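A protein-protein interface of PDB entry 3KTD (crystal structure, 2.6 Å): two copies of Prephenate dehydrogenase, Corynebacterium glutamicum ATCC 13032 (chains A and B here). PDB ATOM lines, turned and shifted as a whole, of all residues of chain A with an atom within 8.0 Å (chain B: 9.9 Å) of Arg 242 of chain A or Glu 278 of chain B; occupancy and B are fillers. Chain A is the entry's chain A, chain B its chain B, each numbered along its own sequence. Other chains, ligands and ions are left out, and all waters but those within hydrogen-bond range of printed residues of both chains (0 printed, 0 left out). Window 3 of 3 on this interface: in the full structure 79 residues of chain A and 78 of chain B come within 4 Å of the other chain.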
ATOM      1  N   THR A  79      -8.071  18.135  -3.534  1.00  0.00           N
ATOM      2  CA  THR A  79      -9.270  18.966  -3.748  1.00  0.00           C
ATOM      3  C   THR A  79     -10.442  18.582  -2.841  1.00  0.00           C
ATOM      4  O   THR A  79     -11.359  19.368  -2.644  1.00  0.00           O
ATOM      5  CB  THR A  79      -9.758  18.927  -5.219  1.00  0.00           C
ATOM      6  OG1 THR A  79     -10.351  17.654  -5.500  1.00  0.00           O
ATOM      7  CG2 THR A  79      -8.601  19.220  -6.201  1.00  0.00           C
ATOM      8  N   VAL A 103       1.264  16.520  -1.304  1.00  0.00           N
ATOM      9  CA  VAL A 103       1.785  17.786  -0.772  1.00  0.00           C
ATOM     10  C   VAL A 103       1.316  17.909   0.672  1.00  0.00           C
ATOM     11  O   VAL A 103       0.202  17.507   0.992  1.00  0.00           O
ATOM     12  CB  VAL A 103       1.284  18.995  -1.590  1.00  0.00           C
ATOM     13  CG1 VAL A 103       1.903  20.286  -1.082  1.00  0.00           C
ATOM     14  CG2 VAL A 103       1.621  18.811  -3.047  1.00  0.00           C
ATOM     15  N   HIS A 202       7.322  14.993 -12.968  1.00  0.00           N
ATOM     16  CA  HIS A 202       6.106  15.130 -13.782  1.00  0.00           C
ATOM     17  C   HIS A 202       6.158  16.290 -14.788  1.00  0.00           C
ATOM     18  O   HIS A 202       5.714  16.125 -15.910  1.00  0.00           O
ATOM     19  CB  HIS A 202       4.866  15.229 -12.894  1.00  0.00           C
ATOM     20  CG  HIS A 202       4.468  13.922 -12.281  1.00  0.00           C
ATOM     21  ND1 HIS A 202       4.698  13.617 -10.958  1.00  0.00           N
ATOM     22  CD2 HIS A 202       3.888  12.827 -12.826  1.00  0.00           C
ATOM     23  CE1 HIS A 202       4.256  12.397 -10.709  1.00  0.00           C
ATOM     24  NE2 HIS A 202       3.765  11.894 -11.827  1.00  0.00           N
ATOM     25  N   ILE A 203       6.711  17.436 -14.395  1.00  0.00           N
ATOM     26  CA  ILE A 203       6.809  18.580 -15.294  1.00  0.00           C
ATOM     27  C   ILE A 203       7.700  18.250 -16.499  1.00  0.00           C
ATOM     28  O   ILE A 203       7.336  18.532 -17.634  1.00  0.00           O
ATOM     29  CB  ILE A 203       7.392  19.813 -14.602  1.00  0.00           C
ATOM     30  CG1 ILE A 203       6.447  20.348 -13.527  1.00  0.00           C
ATOM     31  CG2 ILE A 203       7.634  20.913 -15.615  1.00  0.00           C
ATOM     32  CD1 ILE A 203       5.226  21.046 -14.073  1.00  0.00           C
ATOM     33  N   GLU A 206       5.958  15.848 -18.997  1.00  0.00           N
ATOM     34  CA  GLU A 206       5.016  16.513 -19.903  1.00  0.00           C
ATOM     35  C   GLU A 206       5.803  17.207 -21.030  1.00  0.00           C
ATOM     36  O   GLU A 206       5.476  17.074 -22.214  1.00  0.00           O
ATOM     37  CB  GLU A 206       4.165  17.574 -19.182  1.00  0.00           C
ATOM     38  CG  GLU A 206       3.394  17.146 -17.902  1.00  0.00           C
ATOM     39  CD  GLU A 206       2.239  16.175 -18.127  1.00  0.00           C
ATOM     40  OE1 GLU A 206       2.164  15.508 -19.186  1.00  0.00           O
ATOM     41  OE2 GLU A 206       1.407  16.067 -17.203  1.00  0.00           O
ATOM     42  N   THR A 236      -0.341  10.078 -16.560  1.00  0.00           N
ATOM     43  CA  THR A 236      -1.215  10.303 -15.403  1.00  0.00           C
ATOM     44  C   THR A 236      -2.184  11.444 -15.717  1.00  0.00           C
ATOM     45  O   THR A 236      -2.024  12.177 -16.700  1.00  0.00           O
ATOM     46  CB  THR A 236      -0.486  10.579 -14.047  1.00  0.00           C
ATOM     47  OG1 THR A 236       0.137  11.865 -14.076  1.00  0.00           O
ATOM     48  CG2 THR A 236       0.538   9.482 -13.701  1.00  0.00           C
ATOM     49  N   ASP A 237      -3.195  11.573 -14.873  1.00  0.00           N
ATOM     50  CA  ASP A 237      -4.295  12.475 -15.129  1.00  0.00           C
ATOM     51  C   ASP A 237      -3.896  13.936 -14.996  1.00  0.00           C
ATOM     52  O   ASP A 237      -3.263  14.322 -14.013  1.00  0.00           O
ATOM     53  CB  ASP A 237      -5.440  12.167 -14.172  1.00  0.00           C
ATOM     54  CG  ASP A 237      -6.748  12.706 -14.667  1.00  0.00           C
ATOM     55  OD1 ASP A 237      -6.936  13.948 -14.630  1.00  0.00           O
ATOM     56  OD2 ASP A 237      -7.585  11.881 -15.102  1.00  0.00           O
ATOM     57  N   PRO A 238      -4.277  14.758 -15.985  1.00  0.00           N
ATOM     58  CA  PRO A 238      -3.993  16.183 -15.911  1.00  0.00           C
ATOM     59  C   PRO A 238      -4.492  16.817 -14.611  1.00  0.00           C
ATOM     60  O   PRO A 238      -3.799  17.666 -14.045  1.00  0.00           O
ATOM     61  CB  PRO A 238      -4.742  16.755 -17.114  1.00  0.00           C
ATOM     62  CG  PRO A 238      -4.830  15.638 -18.074  1.00  0.00           C
ATOM     63  CD  PRO A 238      -4.887  14.378 -17.273  1.00  0.00           C
ATOM     64  N   GLY A 239      -5.671  16.409 -14.140  1.00  0.00           N
ATOM     65  CA  GLY A 239      -6.224  16.951 -12.901  1.00  0.00           C
ATOM     66  C   GLY A 239      -5.276  16.765 -11.727  1.00  0.00           C
ATOM     67  O   GLY A 239      -5.055  17.688 -10.934  1.00  0.00           O
ATOM     68  N   LEU A 240      -4.690  15.572 -11.639  1.00  0.00           N
ATOM     69  CA  LEU A 240      -3.765  15.238 -10.547  1.00  0.00           C
ATOM     70  C   LEU A 240      -2.415  15.937 -10.688  1.00  0.00           C
ATOM     71  O   LEU A 240      -1.901  16.482  -9.708  1.00  0.00           O
ATOM     72  CB  LEU A 240      -3.576  13.716 -10.449  1.00  0.00           C
ATOM     73  CG  LEU A 240      -4.901  12.967 -10.242  1.00  0.00           C
ATOM     74  CD1 LEU A 240      -4.683  11.460 -10.071  1.00  0.00           C
ATOM     75  CD2 LEU A 240      -5.666  13.560  -9.050  1.00  0.00           C
ATOM     76  N   VAL A 241      -1.854  15.925 -11.898  1.00  0.00           N
ATOM     77  CA  VAL A 241      -0.564  16.578 -12.157  1.00  0.00           C
ATOM     78  C   VAL A 241      -0.638  18.050 -11.766  1.00  0.00           C
ATOM     79  O   VAL A 241       0.311  18.596 -11.201  1.00  0.00           O
ATOM     80  CB  VAL A 241      -0.129  16.464 -13.637  1.00  0.00           C
ATOM     81  CG1 VAL A 241       1.217  17.135 -13.851  1.00  0.00           C
ATOM     82  CG2 VAL A 241      -0.055  15.012 -14.069  1.00  0.00           C
ATOM     83  N   ARG A 242      -1.776  18.676 -12.052  1.00  0.00           N
ATOM     84  CA  ARG A 242      -2.026  20.071 -11.665  1.00  0.00           C
ATOM     85  C   ARG A 242      -2.172  20.241 -10.160  1.00  0.00           C
ATOM     86  O   ARG A 242      -1.678  21.223  -9.603  1.00  0.00           O
ATOM     87  CB  ARG A 242      -3.291  20.611 -12.336  1.00  0.00           C
ATOM     88  CG  ARG A 242      -3.178  20.843 -13.846  1.00  0.00           C
ATOM     89  CD  ARG A 242      -4.490  21.375 -14.406  1.00  0.00           C
ATOM     90  NE  ARG A 242      -4.824  22.672 -13.817  1.00  0.00           N
ATOM     91  CZ  ARG A 242      -6.033  23.230 -13.832  1.00  0.00           C
ATOM     92  NH1 ARG A 242      -7.064  22.615 -14.412  1.00  0.00           N
ATOM     93  NH2 ARG A 242      -6.216  24.416 -13.259  1.00  0.00           N
ATOM     94  N   ALA A 243      -2.868  19.298  -9.517  1.00  0.00           N
ATOM     95  CA  ALA A 243      -3.087  19.319  -8.060  1.00  0.00           C
ATOM     96  C   ALA A 243      -1.750  19.334  -7.331  1.00  0.00           C
ATOM     97  O   ALA A 243      -1.460  20.279  -6.576  1.00  0.00           O
ATOM     98  CB  ALA A 243      -3.913  18.111  -7.619  1.00  0.00           C
ATOM     99  N   MET A 244      -0.950  18.291  -7.582  1.00  0.00           N
ATOM    100  CA  MET A 244       0.414  18.184  -7.071  1.00  0.00           C
ATOM    101  C   MET A 244       1.161  19.508  -7.214  1.00  0.00           C
ATOM    102  O   MET A 244       1.474  20.186  -6.226  1.00  0.00           O
ATOM    103  CB  MET A 244       1.217  17.153  -7.887  1.00  0.00           C
ATOM    104  CG  MET A 244       0.935  15.672  -7.678  1.00  0.00           C
ATOM    105  SD  MET A 244       2.133  14.723  -8.904  1.00  0.00           S
ATOM    106  CE  MET A 244       1.428  12.883  -8.777  1.00  0.00           C
ATOM    107  N   CYS A 245       1.415  19.881  -8.463  1.00  0.00           N
ATOM    108  CA  CYS A 245       2.282  21.012  -8.768  1.00  0.00           C
ATOM    109  C   CYS A 245       1.776  22.337  -8.264  1.00  0.00           C
ATOM    110  O   CYS A 245       2.561  23.136  -7.753  1.00  0.00           O
ATOM    111  CB  CYS A 245       2.514  21.091 -10.270  1.00  0.00           C
ATOM    112  SG  CYS A 245       3.234  19.573 -10.895  1.00  0.00           S
ATOM    113  N   GLU A 246       0.475  22.575  -8.407  1.00  0.00           N
ATOM    114  CA  GLU A 246      -0.111  23.850  -7.981  1.00  0.00           C
ATOM    115  C   GLU A 246      -0.117  23.969  -6.457  1.00  0.00           C
ATOM    116  O   GLU A 246       0.222  25.025  -5.916  1.00  0.00           O
ATOM    117  CB  GLU A 246      -1.504  24.040  -8.586  1.00  0.00           C
ATOM    118  CG  GLU A 246      -1.461  24.254 -10.099  1.00  0.00           C
ATOM    119  CD  GLU A 246      -2.786  24.029 -10.802  1.00  0.00           C
ATOM    120  OE1 GLU A 246      -3.682  23.377 -10.231  1.00  0.00           O
ATOM    121  OE2 GLU A 246      -2.926  24.490 -11.951  1.00  0.00           O
ATOM    122  N   SER A 247      -0.467  22.877  -5.773  1.00  0.00           N
ATOM    123  CA  SER A 247      -0.399  22.818  -4.300  1.00  0.00           C
ATOM    124  C   SER A 247       0.997  23.160  -3.779  1.00  0.00           C
ATOM    125  O   SER A 247       1.132  23.775  -2.728  1.00  0.00           O
ATOM    126  CB  SER A 247      -0.740  21.413  -3.794  1.00  0.00           C
ATOM    127  OG  SER A 247      -2.016  20.975  -4.227  1.00  0.00           O
ATOM    128  N   ASN A 248       2.024  22.751  -4.524  1.00  0.00           N
ATOM    129  CA  ASN A 248       3.416  22.912  -4.113  1.00  0.00           C
ATOM    130  C   ASN A 248       4.225  23.812  -5.062  1.00  0.00           C
ATOM    131  O   ASN A 248       5.411  23.587  -5.288  1.00  0.00           O
ATOM    132  CB  ASN A 248       4.051  21.514  -4.034  1.00  0.00           C
ATOM    133  CG  ASN A 248       5.327  21.485  -3.227  1.00  0.00           C
ATOM    134  OD1 ASN A 248       5.525  22.294  -2.323  1.00  0.00           O
ATOM    135  ND2 ASN A 248       6.199  20.535  -3.544  1.00  0.00           N
ATOM    136  N   ALA A 249       3.582  24.847  -5.595  1.00  0.00           N
ATOM    137  CA  ALA A 249       4.214  25.749  -6.556  1.00  0.00           C
ATOM    138  C   ALA A 249       5.496  26.392  -6.036  1.00  0.00           C
ATOM    139  O   ALA A 249       6.479  26.514  -6.771  1.00  0.00           O
ATOM    140  CB  ALA A 249       3.236  26.820  -6.966  1.00  0.00           C
ATOM    141  N   LEU A 252       8.355  23.913  -5.803  1.00  0.00           N
ATOM    142  CA  LEU A 252       8.544  23.421  -7.178  1.00  0.00           C
ATOM    143  C   LEU A 252       9.317  24.423  -8.039  1.00  0.00           C
ATOM    144  O   LEU A 252      10.197  24.033  -8.801  1.00  0.00           O
ATOM    145  CB  LEU A 252       7.216  23.068  -7.857  1.00  0.00           C
ATOM    146  CG  LEU A 252       7.317  22.508  -9.291  1.00  0.00           C
ATOM    147  CD1 LEU A 252       8.416  21.449  -9.426  1.00  0.00           C
ATOM    148  CD2 LEU A 252       5.983  21.940  -9.769  1.00  0.00           C
ATOM    149  N   ILE B 262       8.765  25.650 -23.126  1.00  0.00           N
ATOM    150  CA  ILE B 262       7.697  25.000 -22.366  1.00  0.00           C
ATOM    151  C   ILE B 262       7.916  25.119 -20.859  1.00  0.00           C
ATOM    152  O   ILE B 262       6.993  25.423 -20.110  1.00  0.00           O
ATOM    153  CB  ILE B 262       7.596  23.510 -22.736  1.00  0.00           C
ATOM    154  CG1 ILE B 262       7.129  23.356 -24.182  1.00  0.00           C
ATOM    155  CG2 ILE B 262       6.634  22.797 -21.811  1.00  0.00           C
ATOM    156  CD1 ILE B 262       7.344  21.979 -24.730  1.00  0.00           C
ATOM    157  N   GLU B 265       7.334  28.768 -19.675  1.00  0.00           N
ATOM    158  CA  GLU B 265       5.889  29.004 -19.735  1.00  0.00           C
ATOM    159  C   GLU B 265       5.173  28.315 -18.568  1.00  0.00           C
ATOM    160  O   GLU B 265       4.148  28.794 -18.100  1.00  0.00           O
ATOM    161  CB  GLU B 265       5.315  28.540 -21.086  1.00  0.00           C
ATOM    162  CG  GLU B 265       3.895  29.027 -21.383  1.00  0.00           C
ATOM    163  N   ALA B 266       5.723  27.194 -18.109  1.00  0.00           N
ATOM    164  CA  ALA B 266       5.211  26.485 -16.939  1.00  0.00           C
ATOM    165  C   ALA B 266       5.555  27.243 -15.647  1.00  0.00           C
ATOM    166  O   ALA B 266       4.746  27.308 -14.707  1.00  0.00           O
ATOM    167  CB  ALA B 266       5.789  25.097 -16.896  1.00  0.00           C
ATOM    168  N   ARG B 267       6.762  27.805 -15.604  1.00  0.00           N
ATOM    169  CA  ARG B 267       7.198  28.601 -14.461  1.00  0.00           C
ATOM    170  C   ARG B 267       6.372  29.882 -14.360  1.00  0.00           C
ATOM    171  O   ARG B 267       6.064  30.346 -13.259  1.00  0.00           O
ATOM    172  CB  ARG B 267       8.679  28.949 -14.571  1.00  0.00           C
ATOM    173  CG  ARG B 267       9.235  29.574 -13.301  1.00  0.00           C
ATOM    174  CD  ARG B 267      10.592  30.190 -13.526  1.00  0.00           C
ATOM    175  NE  ARG B 267      11.217  30.584 -12.265  1.00  0.00           N
ATOM    176  CZ  ARG B 267      10.937  31.694 -11.586  1.00  0.00           C
ATOM    177  NH1 ARG B 267      10.004  32.537 -12.015  1.00  0.00           N
ATOM    178  NH2 ARG B 267      11.586  31.951 -10.456  1.00  0.00           N
ATOM    179  N   GLU B 268       6.033  30.461 -15.510  1.00  0.00           N
ATOM    180  CA  GLU B 268       5.133  31.606 -15.545  1.00  0.00           C
ATOM    181  C   GLU B 268       3.866  31.138 -14.846  1.00  0.00           C
ATOM    182  O   GLU B 268       3.355  31.812 -13.955  1.00  0.00           O
ATOM    183  N   GLY B 269       3.396  29.953 -15.236  1.00  0.00           N
ATOM    184  CA  GLY B 269       2.206  29.342 -14.652  1.00  0.00           C
ATOM    185  C   GLY B 269       2.217  29.111 -13.143  1.00  0.00           C
ATOM    186  O   GLY B 269       1.208  29.323 -12.476  1.00  0.00           O
ATOM    187  N   LEU B 270       3.348  28.678 -12.595  1.00  0.00           N
ATOM    188  CA  LEU B 270       3.433  28.355 -11.162  1.00  0.00           C
ATOM    189  C   LEU B 270       3.722  29.565 -10.271  1.00  0.00           C
ATOM    190  O   LEU B 270       3.610  29.471  -9.045  1.00  0.00           O
ATOM    191  CB  LEU B 270       4.497  27.284 -10.930  1.00  0.00           C
ATOM    192  CG  LEU B 270       4.229  25.935 -11.603  1.00  0.00           C
ATOM    193  CD1 LEU B 270       5.521  25.135 -11.750  1.00  0.00           C
ATOM    194  CD2 LEU B 270       3.181  25.162 -10.822  1.00  0.00           C
ATOM    195  N   GLN B 274      -2.663  32.954  -8.799  1.00  0.00           N
ATOM    196  CA  GLN B 274      -3.259  31.629  -8.677  1.00  0.00           C
ATOM    197  C   GLN B 274      -2.526  30.641  -9.600  1.00  0.00           C
ATOM    198  O   GLN B 274      -2.866  30.534 -10.780  1.00  0.00           O
ATOM    199  CB  GLN B 274      -4.748  31.680  -9.019  1.00  0.00           C
ATOM    200  CG  GLN B 274      -5.475  30.348  -8.796  1.00  0.00           C
ATOM    201  CD  GLN B 274      -6.996  30.489  -8.738  1.00  0.00           C
ATOM    202  OE1 GLN B 274      -7.721  29.658  -9.284  1.00  0.00           O
ATOM    203  NE2 GLN B 274      -7.485  31.540  -8.074  1.00  0.00           N
ATOM    204  N   PRO B 275      -1.509  29.929  -9.065  1.00  0.00           N
ATOM    205  CA  PRO B 275      -0.728  28.942  -9.808  1.00  0.00           C
ATOM    206  C   PRO B 275      -1.561  28.075 -10.744  1.00  0.00           C
ATOM    207  O   PRO B 275      -2.570  27.502 -10.324  1.00  0.00           O
ATOM    208  CB  PRO B 275      -0.115  28.095  -8.698  1.00  0.00           C
ATOM    209  CG  PRO B 275       0.147  29.069  -7.627  1.00  0.00           C
ATOM    210  CD  PRO B 275      -0.981  30.084  -7.697  1.00  0.00           C
ATOM    211  N   ASN B 276      -1.115  27.981 -11.997  1.00  0.00           N
ATOM    212  CA  ASN B 276      -1.848  27.280 -13.048  1.00  0.00           C
ATOM    213  C   ASN B 276      -0.938  26.696 -14.145  1.00  0.00           C
ATOM    214  O   ASN B 276      -0.254  27.447 -14.840  1.00  0.00           O
ATOM    215  CB  ASN B 276      -2.859  28.253 -13.676  1.00  0.00           C
ATOM    216  CG  ASN B 276      -3.837  27.574 -14.631  1.00  0.00           C
ATOM    217  OD1 ASN B 276      -3.632  26.440 -15.065  1.00  0.00           O
ATOM    218  ND2 ASN B 276      -4.909  28.280 -14.964  1.00  0.00           N
ATOM    219  N   ILE B 277      -0.942  25.364 -14.284  1.00  0.00           N
ATOM    220  CA  ILE B 277      -0.248  24.674 -15.383  1.00  0.00           C
ATOM    221  C   ILE B 277      -1.234  23.832 -16.200  1.00  0.00           C
ATOM    222  O   ILE B 277      -0.950  22.693 -16.574  1.00  0.00           O
ATOM    223  CB  ILE B 277       0.955  23.802 -14.910  1.00  0.00           C
ATOM    224  CG1 ILE B 277       0.519  22.713 -13.922  1.00  0.00           C
ATOM    225  CG2 ILE B 277       2.031  24.679 -14.280  1.00  0.00           C
ATOM    226  CD1 ILE B 277       1.521  21.584 -13.786  1.00  0.00           C
ATOM    227  N   GLU B 278      -2.409  24.405 -16.454  1.00  0.00           N
ATOM    228  CA  GLU B 278      -3.401  23.793 -17.334  1.00  0.00           C
ATOM    229  C   GLU B 278      -2.724  23.315 -18.610  1.00  0.00           C
ATOM    230  O   GLU B 278      -2.624  22.116 -18.880  1.00  0.00           O
ATOM    231  CB  GLU B 278      -4.472  24.822 -17.728  1.00  0.00           C
ATOM    232  CG  GLU B 278      -5.753  24.787 -16.929  1.00  0.00           C
ATOM    233  CD  GLU B 278      -6.711  23.711 -17.426  1.00  0.00           C
ATOM    234  OE1 GLU B 278      -6.307  22.524 -17.479  1.00  0.00           O
ATOM    235  OE2 GLU B 278      -7.866  24.061 -17.760  1.00  0.00           O
ATOM    236  N   GLN B 279      -2.250  24.305 -19.360  1.00  0.00           N
ATOM    237  CA  GLN B 279      -1.654  24.138 -20.674  1.00  0.00           C
ATOM    238  C   GLN B 279      -0.682  22.960 -20.735  1.00  0.00           C
ATOM    239  O   GLN B 279      -0.864  22.039 -21.538  1.00  0.00           O
ATOM    240  CB  GLN B 279      -0.965  25.453 -21.072  1.00  0.00           C
ATOM    241  CG  GLN B 279      -0.342  25.478 -22.466  1.00  0.00           C
ATOM    242  CD  GLN B 279      -0.075  26.899 -22.967  1.00  0.00           C
ATOM    243  OE1 GLN B 279      -0.880  27.813 -22.753  1.00  0.00           O
ATOM    244  NE2 GLN B 279       1.050  27.084 -23.654  1.00  0.00           N
ATOM    245  N   LEU B 280       0.325  22.981 -19.864  1.00  0.00           N
ATOM    246  CA  LEU B 280       1.349  21.942 -19.846  1.00  0.00           C
ATOM    247  C   LEU B 280       0.762  20.555 -19.634  1.00  0.00           C
ATOM    248  O   LEU B 280       1.016  19.640 -20.421  1.00  0.00           O
ATOM    249  CB  LEU B 280       2.380  22.223 -18.754  1.00  0.00           C
ATOM    250  CG  LEU B 280       3.591  21.286 -18.770  1.00  0.00           C
ATOM    251  CD1 LEU B 280       4.273  21.362 -20.121  1.00  0.00           C
ATOM    252  CD2 LEU B 280       4.563  21.616 -17.647  1.00  0.00           C
ATOM    253  N   ALA B 281      -0.012  20.408 -18.564  1.00  0.00           N
ATOM    254  CA  ALA B 281      -0.632  19.133 -18.217  1.00  0.00           C
ATOM    255  C   ALA B 281      -1.470  18.581 -19.369  1.00  0.00           C
ATOM    256  O   ALA B 281      -1.294  17.430 -19.769  1.00  0.00           O
ATOM    257  CB  ALA B 281      -1.482  19.290 -16.971  1.00  0.00           C
ATOM    258  N   ASP B 282      -2.355  19.412 -19.914  1.00  0.00           N
ATOM    259  CA  ASP B 282      -3.229  19.010 -21.030  1.00  0.00           C
ATOM    260  C   ASP B 282      -2.451  18.579 -22.300  1.00  0.00           C
ATOM    261  O   ASP B 282      -2.668  17.485 -22.834  1.00  0.00           O
ATOM    262  CB  ASP B 282      -4.195  20.147 -21.397  1.00  0.00           C
ATOM    263  CG  ASP B 282      -5.026  20.638 -20.212  1.00  0.00           C
ATOM    264  OD1 ASP B 282      -5.096  19.942 -19.172  1.00  0.00           O
ATOM    265  OD2 ASP B 282      -5.609  21.741 -20.325  1.00  0.00           O
ATOM    266  N   ASN B 283      -1.559  19.445 -22.782  1.00  0.00           N
ATOM    267  CA  ASN B 283      -0.763  19.156 -23.978  1.00  0.00           C
ATOM    268  C   ASN B 283       0.132  17.962 -23.729  1.00  0.00           C
ATOM    269  O   ASN B 283       0.327  17.115 -24.610  1.00  0.00           O
ATOM    270  CB  ASN B 283       0.110  20.352 -24.360  1.00  0.00           C
ATOM    271  CG  ASN B 283      -0.697  21.578 -24.704  1.00  0.00           C
ATOM    272  OD1 ASN B 283      -1.893  21.496 -24.979  1.00  0.00           O
ATOM    273  ND2 ASN B 283      -0.046  22.730 -24.683  1.00  0.00           N
ATOM    274  N   GLY B 284       0.689  17.908 -22.523  1.00  0.00           N
ATOM    275  CA  GLY B 284       1.525  16.791 -22.127  1.00  0.00           C
ATOM    276  C   GLY B 284       0.736  15.502 -22.180  1.00  0.00           C
ATOM    277  O   GLY B 284       1.092  14.583 -22.908  1.00  0.00           O
ATOM    278  N   TYR B 285      -0.352  15.449 -21.418  1.00  0.00           N
ATOM    279  CA  TYR B 285      -1.200  14.259 -21.379  1.00  0.00           C
ATOM    280  C   TYR B 285      -1.651  13.841 -22.771  1.00  0.00           C
ATOM    281  O   TYR B 285      -1.531  12.672 -23.148  1.00  0.00           O
ATOM    282  CB  TYR B 285      -2.415  14.492 -20.476  1.00  0.00           C
ATOM    283  CG  TYR B 285      -3.447  13.381 -20.523  1.00  0.00           C
ATOM    284  CD1 TYR B 285      -3.234  12.165 -19.867  1.00  0.00           C
ATOM    285  CD2 TYR B 285      -4.644  13.552 -21.221  1.00  0.00           C
ATOM    286  CE1 TYR B 285      -4.186  11.145 -19.915  1.00  0.00           C
ATOM    287  CE2 TYR B 285      -5.601  12.547 -21.270  1.00  0.00           C
ATOM    288  CZ  TYR B 285      -5.374  11.347 -20.615  1.00  0.00           C
ATOM    289  OH  TYR B 285      -6.333  10.357 -20.669  1.00  0.00           O
ATOM    290  N   ARG B 286      -2.146  14.809 -23.537  1.00  0.00           N
ATOM    291  CA  ARG B 286      -2.604  14.538 -24.888  1.00  0.00           C
ATOM    292  C   ARG B 286      -1.466  14.056 -25.792  1.00  0.00           C
ATOM    293  O   ARG B 286      -1.697  13.224 -26.662  1.00  0.00           O
ATOM    294  CB  ARG B 286      -3.307  15.762 -25.483  1.00  0.00           C
ATOM    295  CG  ARG B 286      -4.263  15.416 -26.635  1.00  0.00           C
ATOM    296  CD  ARG B 286      -5.362  16.457 -26.791  1.00  0.00           C
ATOM    297  NE  ARG B 286      -6.093  16.653 -25.539  1.00  0.00           N
ATOM    298  CZ  ARG B 286      -7.084  17.527 -25.369  1.00  0.00           C
ATOM    299  NH1 ARG B 286      -7.489  18.288 -26.379  1.00  0.00           N
ATOM    300  NH2 ARG B 286      -7.684  17.631 -24.183  1.00  0.00           N
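OE1 of Glu 206 of chain A lies within hydrogen-bond range of N of Tyr 285 of chain B (3.4 Å). NH1 of Arg 242 of chain A is in salt-bridge range of OE1 of Glu 278 of chain B (3.2 Å). The backbone NH (N) of Ile 277 of chain B is in hydrogen-bond range of the side-chain carboxylate (OE2) of Glu 246 of chain A (3.2 Å). OE2 of Glu 246 of chain A sits close to O of Pro 275 of chain B (3.4 Å).
SG of Cys 245 of chain A sits at hydrogen-bond distance from O of Val 241 of chain A (3.1 Å). The guanidinium group of Arg 242 of chain A is in salt-bridge range of the side-chain carboxylate of Glu 246 of chain A, 3.2 Å away. O of Gly 269 of chain B is in hydrogen-bond range of N of Asn 276 of chain B, 2.7 Å away. The side-chain amide oxygen (OD1) of Asn 276 of chain B lies within hydrogen-bond range of the backbone NH (N) of Glu 278 of chain B, 2.8 Å away.
CD1 of Ile 203 of chain A touches CD1 of Ile 277 of chain B (3.8 Å). Leu 280 of chain B touches Ile 203 of chain A. Glu 206 of chain A touches Gly 284 of chain B (OE1 to CA, 3.3 Å). Thr 236 of chain A touches Tyr 285 of chain B. Asp 282 of chain B touches Pro 238 of chain A (OD1 to CB, 3.8 Å). OD1 of Asn 276 of chain B touches NH2 of Arg 242 of chain A, at 3.7 Å. Arg 242 of chain A touches Ile 277 of chain B (CG to O, 3.98 Å). CD2 of Leu 270 of chain B touches O of Cys 245 of chain A, 3.7 Å away. Cys 245 of chain A touches Ile 277 of chain B. Leu 252 of chain A touches Leu 270 of chain B (CD2 to CD1, 3.8 Å).
Arg 242 of chain A touches just these residues of chain B: Asn 276 (3.7 Å), Ile 277 (3.98 Å), Glu 278 (3.2 Å) and Ala 281 (3.9 Å). Glu 278 of chain B touches just one residue of chain A: Arg 242. No residue of chain B comes within 4 Å of Gly 239 of chain A. Val 241 of chain A touches none of the printed residues of chain B. No residue of chain B comes within 4 Å of Ala 243 of chain A. Of chain B, only Leu 270 (3.7 Å) and Ile 277 (3.7 Å) come within 4 Å of Cys 245 of chain A. Printed residues of chain B within 4 Å of Pro 238 of chain A: Asp 282 and Tyr 285. Of the printed residues of chain A, Gly 284 of chain B touches Glu 206 (3.3 Å). Val 103 of chain A touches none of the printed residues of chain B. Asn 283 of chain B touches none of the printed residues of chain A. The nearest printed residue of chain B that does not touch Leu 252 of chain A is Ile 277 of chain B (6.0 Å).
Hydrophobic or aromatic side chains of chain A within 4 Å of the printed part of chain B: Ile 203, Pro 238, Ala 249 and Leu 252. Of the 20 printed residues of chain B, 10 touch a printed residue of chain A. Hydrophobic or aromatic side chains of chain B that line the printed part of chain A: Leu 270, Pro 275, Ile 277, Leu 280, Ala 281 and Tyr 285. Among the printed residues, Asp or Glu carboxylates within 4 Å of a Lys or Arg side-chain nitrogen of the other chain: Arg 242 of chain A with Glu 278 of chain B (3.2 Å).
No position is printed for both chains. Of the 21 pairs that touch across the chains among the printed residues, none has its exchanged pair printed and touching as well.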
